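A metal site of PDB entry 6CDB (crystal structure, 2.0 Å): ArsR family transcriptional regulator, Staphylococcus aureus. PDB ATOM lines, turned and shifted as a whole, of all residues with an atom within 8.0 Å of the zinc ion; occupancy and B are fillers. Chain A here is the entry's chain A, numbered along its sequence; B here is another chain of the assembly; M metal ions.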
ATOM      1  N   GLN A  93      20.022   9.960  27.902  1.00  0.00           N
ATOM      2  CA  GLN A  93      20.930   8.971  27.322  1.00  0.00           C
ATOM      3  C   GLN A  93      22.163   8.774  28.192  1.00  0.00           C
ATOM      4  O   GLN A  93      22.616   7.642  28.390  1.00  0.00           O
ATOM      5  CB  GLN A  93      21.351   9.372  25.895  1.00  0.00           C
ATOM      6  CG  GLN A  93      20.180   9.389  24.889  1.00  0.00           C
ATOM      7  CD  GLN A  93      19.863   8.017  24.306  1.00  0.00           C
ATOM      8  OE1 GLN A  93      20.769   7.255  23.976  1.00  0.00           O
ATOM      9  NE2 GLN A  93      18.561   7.706  24.167  1.00  0.00           N
ATOM     10  N   ALA A  94      22.721   9.876  28.719  1.00  0.00           N
ATOM     11  CA  ALA A  94      23.861   9.760  29.625  1.00  0.00           C
ATOM     12  C   ALA A  94      23.507   8.973  30.892  1.00  0.00           C
ATOM     13  O   ALA A  94      24.270   8.112  31.328  1.00  0.00           O
ATOM     14  CB  ALA A  94      24.395  11.151  29.985  1.00  0.00           C
ATOM     15  N   ILE A  95      22.347   9.267  31.490  1.00  0.00           N
ATOM     16  CA  ILE A  95      21.939   8.571  32.719  1.00  0.00           C
ATOM     17  C   ILE A  95      21.779   7.080  32.448  1.00  0.00           C
ATOM     18  O   ILE A  95      22.283   6.239  33.202  1.00  0.00           O
ATOM     19  CB  ILE A  95      20.636   9.188  33.270  1.00  0.00           C
ATOM     20  CG1 ILE A  95      20.887  10.616  33.754  1.00  0.00           C
ATOM     21  CG2 ILE A  95      20.053   8.339  34.409  1.00  0.00           C
ATOM     22  CD1 ILE A  95      19.627  11.341  34.191  1.00  0.00           C
ATOM     23  N   HIS A  96      21.104   6.737  31.333  1.00  0.00           N
ATOM     24  CA  HIS A  96      20.927   5.331  31.004  1.00  0.00           C
ATOM     25  C   HIS A  96      22.263   4.645  30.775  1.00  0.00           C
ATOM     26  O   HIS A  96      22.466   3.504  31.193  1.00  0.00           O
ATOM     27  CB  HIS A  96      20.048   5.179  29.769  1.00  0.00           C
ATOM     28  CG  HIS A  96      19.915   3.765  29.306  1.00  0.00           C
ATOM     29  ND1 HIS A  96      19.018   2.881  29.862  1.00  0.00           N
ATOM     30  CD2 HIS A  96      20.562   3.087  28.328  1.00  0.00           C
ATOM     31  CE1 HIS A  96      19.123   1.709  29.261  1.00  0.00           C
ATOM     32  NE2 HIS A  96      20.043   1.807  28.318  1.00  0.00           N
ATOM     33  N   HIS A  97      23.182   5.333  30.077  1.00  0.00           N
ATOM     34  CA  HIS A  97      24.488   4.755  29.804  1.00  0.00           C
ATOM     35  C   HIS A  97      25.260   4.505  31.099  1.00  0.00           C
ATOM     36  O   HIS A  97      25.924   3.474  31.261  1.00  0.00           O
ATOM     37  CB  HIS A  97      25.283   5.670  28.882  1.00  0.00           C
ATOM     38  CG  HIS A  97      26.593   5.103  28.441  1.00  0.00           C
ATOM     39  ND1 HIS A  97      26.684   4.018  27.586  1.00  0.00           N
ATOM     40  CD2 HIS A  97      27.866   5.439  28.751  1.00  0.00           C
ATOM     41  CE1 HIS A  97      27.959   3.738  27.376  1.00  0.00           C
ATOM     42  NE2 HIS A  97      28.699   4.591  28.072  1.00  0.00           N
ATOM     43  N   ALA A  98      25.218   5.472  32.016  1.00  0.00           N
ATOM     44  CA  ALA A  98      25.808   5.248  33.338  1.00  0.00           C
ATOM     45  C   ALA A  98      25.173   4.055  34.029  1.00  0.00           C
ATOM     46  O   ALA A  98      25.854   3.299  34.732  1.00  0.00           O
ATOM     47  CB  ALA A  98      25.642   6.499  34.198  1.00  0.00           C
ATOM     48  N   ASN A  99      23.878   3.842  33.812  1.00  0.00           N
ATOM     49  CA  ASN A  99      23.176   2.823  34.595  1.00  0.00           C
ATOM     50  C   ASN A  99      23.378   1.414  34.050  1.00  0.00           C
ATOM     51  O   ASN A  99      23.565   0.481  34.839  1.00  0.00           O
ATOM     52  CB  ASN A  99      21.687   3.155  34.644  1.00  0.00           C
ATOM     53  CG  ASN A  99      21.184   3.219  36.056  1.00  0.00           C
ATOM     54  OD1 ASN A  99      21.797   2.666  36.967  1.00  0.00           O
ATOM     55  ND2 ASN A  99      20.067   3.899  36.249  1.00  0.00           N
ATOM     56  N   HIS A 100      23.310   1.217  32.736  1.00  0.00           N
ATOM     57  CA  HIS A 100      23.238  -0.135  32.204  1.00  0.00           C
ATOM     58  C   HIS A 100      24.571  -0.864  32.410  1.00  0.00           C
ATOM     59  O   HIS A 100      25.618  -0.237  32.589  1.00  0.00           O
ATOM     60  CB  HIS A 100      22.800  -0.121  30.732  1.00  0.00           C
ATOM     61  CG  HIS A 100      23.822   0.388  29.762  1.00  0.00           C
ATOM     62  ND1 HIS A 100      25.000  -0.286  29.491  1.00  0.00           N
ATOM     63  CD2 HIS A 100      23.814   1.457  28.935  1.00  0.00           C
ATOM     64  CE1 HIS A 100      25.690   0.373  28.571  1.00  0.00           C
ATOM     65  NE2 HIS A 100      24.983   1.435  28.213  1.00  0.00           N
ATOM     66  N   PRO A 101      24.535  -2.196  32.461  1.00  0.00           N
ATOM     67  CA  PRO A 101      25.757  -2.955  32.719  1.00  0.00           C
ATOM     68  C   PRO A 101      26.752  -2.818  31.587  1.00  0.00           C
ATOM     69  O   PRO A 101      26.428  -2.415  30.471  1.00  0.00           O
ATOM     70  CB  PRO A 101      25.267  -4.400  32.848  1.00  0.00           C
ATOM     71  CG  PRO A 101      23.798  -4.294  33.125  1.00  0.00           C
ATOM     72  CD  PRO A 101      23.352  -3.075  32.388  1.00  0.00           C
ATOM     73  N   LYS A 102      28.000  -3.179  31.886  1.00  0.00           N
ATOM     74  CA  LYS A 102      29.087  -3.076  30.928  1.00  0.00           C
ATOM     75  C   LYS A 102      29.769  -4.421  30.726  1.00  0.00           C
ATOM     76  O   LYS A 102      30.489  -4.623  29.745  1.00  0.00           O
ATOM     77  CB  LYS A 102      30.105  -2.027  31.404  1.00  0.00           C
ATOM     78  CG  LYS A 102      29.510  -0.683  31.812  1.00  0.00           C
ATOM     79  CD  LYS A 102      28.931   0.084  30.616  1.00  0.00           C
ATOM     80  CE  LYS A 102      28.499   1.483  31.029  1.00  0.00           C
ATOM     81  NZ  LYS A 102      27.467   1.450  32.111  1.00  0.00           N
ATOM     82  N   HIS B  67      33.950   4.349  30.059  1.00  0.00           N
ATOM     83  CA  HIS B  67      33.099   3.676  29.087  1.00  0.00           C
ATOM     84  C   HIS B  67      32.522   4.647  28.067  1.00  0.00           C
ATOM     85  O   HIS B  67      31.392   4.495  27.605  1.00  0.00           O
ATOM     86  CB  HIS B  67      31.966   2.899  29.764  1.00  0.00           C
ATOM     87  CG  HIS B  67      32.462   1.873  30.731  1.00  0.00           C
ATOM     88  ND1 HIS B  67      33.075   0.703  30.329  1.00  0.00           N
ATOM     89  CD2 HIS B  67      32.467   1.842  32.082  1.00  0.00           C
ATOM     90  CE1 HIS B  67      33.431   0.002  31.383  1.00  0.00           C
ATOM     91  NE2 HIS B  67      33.072   0.678  32.465  1.00  0.00           N
ATOM     92  N   ASP B  83      31.713   4.422  22.557  1.00  0.00           N
ATOM     93  CA  ASP B  83      31.470   3.130  23.194  1.00  0.00           C
ATOM     94  C   ASP B  83      30.195   2.469  22.674  1.00  0.00           C
ATOM     95  O   ASP B  83      30.227   1.302  22.262  1.00  0.00           O
ATOM     96  CB  ASP B  83      31.404   3.296  24.711  1.00  0.00           C
ATOM     97  CG  ASP B  83      31.009   2.003  25.428  1.00  0.00           C
ATOM     98  OD1 ASP B  83      31.917   1.205  25.748  1.00  0.00           O
ATOM     99  OD2 ASP B  83      29.784   1.770  25.642  1.00  0.00           O
ATOM    100  N   ASP B  84      29.073   3.182  22.676  1.00  0.00           N
ATOM    101  CA  ASP B  84      27.829   2.636  22.139  1.00  0.00           C
ATOM    102  C   ASP B  84      26.944   3.780  21.676  1.00  0.00           C
ATOM    103  O   ASP B  84      27.357   4.947  21.653  1.00  0.00           O
ATOM    104  CB  ASP B  84      27.140   1.714  23.164  1.00  0.00           C
ATOM    105  CG  ASP B  84      26.594   2.466  24.398  1.00  0.00           C
ATOM    106  OD1 ASP B  84      26.284   1.800  25.419  1.00  0.00           O
ATOM    107  OD2 ASP B  84      26.466   3.707  24.369  1.00  0.00           O
ATOM    108  N   ILE B  85      25.701   3.451  21.324  1.00  0.00           N
ATOM    109  CA  ILE B  85      24.806   4.433  20.716  1.00  0.00           C
ATOM    110  C   ILE B  85      24.395   5.534  21.704  1.00  0.00           C
ATOM    111  O   ILE B  85      24.033   6.638  21.296  1.00  0.00           O
ATOM    112  CB  ILE B  85      23.574   3.719  20.131  1.00  0.00           C
ATOM    113  CG1 ILE B  85      22.819   4.695  19.235  1.00  0.00           C
ATOM    114  CG2 ILE B  85      22.669   3.216  21.266  1.00  0.00           C
ATOM    115  CD1 ILE B  85      21.355   4.397  19.128  1.00  0.00           C
ATOM    116  N   HIS B  86      24.377   5.248  23.010  1.00  0.00           N
ATOM    117  CA  HIS B  86      24.027   6.302  23.959  1.00  0.00           C
ATOM    118  C   HIS B  86      25.075   7.409  23.957  1.00  0.00           C
ATOM    119  O   HIS B  86      24.736   8.590  24.054  1.00  0.00           O
ATOM    120  CB  HIS B  86      23.871   5.718  25.373  1.00  0.00           C
ATOM    121  CG  HIS B  86      23.027   4.476  25.399  1.00  0.00           C
ATOM    122  ND1 HIS B  86      23.521   3.260  25.834  1.00  0.00           N
ATOM    123  CD2 HIS B  86      21.764   4.246  25.000  1.00  0.00           C
ATOM    124  CE1 HIS B  86      22.573   2.348  25.727  1.00  0.00           C
ATOM    125  NE2 HIS B  86      21.504   2.918  25.215  1.00  0.00           N
ATOM    126  N   VAL B  87      26.351   7.028  23.872  1.00  0.00           N
ATOM    127  CA  VAL B  87      27.420   8.023  23.841  1.00  0.00           C
ATOM    128  C   VAL B  87      27.349   8.842  22.564  1.00  0.00           C
ATOM    129  O   VAL B  87      27.399  10.084  22.595  1.00  0.00           O
ATOM    130  CB  VAL B  87      28.781   7.341  24.030  1.00  0.00           C
ATOM    131  CG1 VAL B  87      29.919   8.369  24.030  1.00  0.00           C
ATOM    132  CG2 VAL B  87      28.790   6.543  25.332  1.00  0.00           C
ATOM    133  N   ALA B  88      27.185   8.171  21.417  1.00  0.00           N
ATOM    134  CA  ALA B  88      27.043   8.882  20.149  1.00  0.00           C
ATOM    135  C   ALA B  88      25.844   9.823  20.180  1.00  0.00           C
ATOM    136  O   ALA B  88      25.924  10.963  19.714  1.00  0.00           O
ATOM    137  CB  ALA B  88      26.915   7.896  18.983  1.00  0.00           C
ATOM    138  N   MET B  90      24.149  11.162  22.876  1.00  0.00           N
ATOM    139  CA  MET B  90      24.478  12.260  23.786  1.00  0.00           C
ATOM    140  C   MET B  90      25.317  13.332  23.092  1.00  0.00           C
ATOM    141  O   MET B  90      24.967  14.517  23.113  1.00  0.00           O
ATOM    142  CB  MET B  90      25.210  11.693  24.998  1.00  0.00           C
ATOM    143  CG  MET B  90      25.651  12.716  26.035  1.00  0.00           C
ATOM    144  SD  MET B  90      26.791  11.973  27.211  1.00  0.00           S
ATOM    145  CE  MET B  90      26.351  10.244  27.003  1.00  0.00           C
HETATM  146 ZN    ZN M   1      25.315   2.783  26.700  1.00  0.00          ZN
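Four residues have an atom within 4 Å of the zinc ion: His 97, His 100, Asp 84 of chain B and His 86 of chain B. The nearest printed residue that does not touch the zinc ion is Asp 83 of chain B (4.7 Å).
A ring nitrogen (NE2) of His 97 lies within hydrogen-bond range of the backbone carbonyl oxygen (O) of His 67 of chain B. The backbone carbonyl oxygen (O) of His 97 lies within hydrogen-bond range of the side-chain amino group (NZ) of Lys 102 (2.7 Å). The side-chain carboxylate (OD2) of Asp 84 of chain B is in hydrogen-bond range of the backbone NH (N) of Val 87 of chain B (3.4 Å). The backbone carbonyl oxygen of His 100 lies within hydrogen-bond range of the side-chain amino group of Lys 102.
The zinc ion is bound by the side-chain carboxylate (OD1) of Asp 84 of chain B (1.9 Å), a ring nitrogen (ND1) of His 97 (2.0 Å), a ring nitrogen (ND1) of His 86 of chain B (2.0 Å) and a ring nitrogen (NE2) of His 100 (2.1 Å). Slightly farther from the zinc ion lies the side-chain carboxylate (OD2) of Asp 84 of chain B (2.8 Å).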
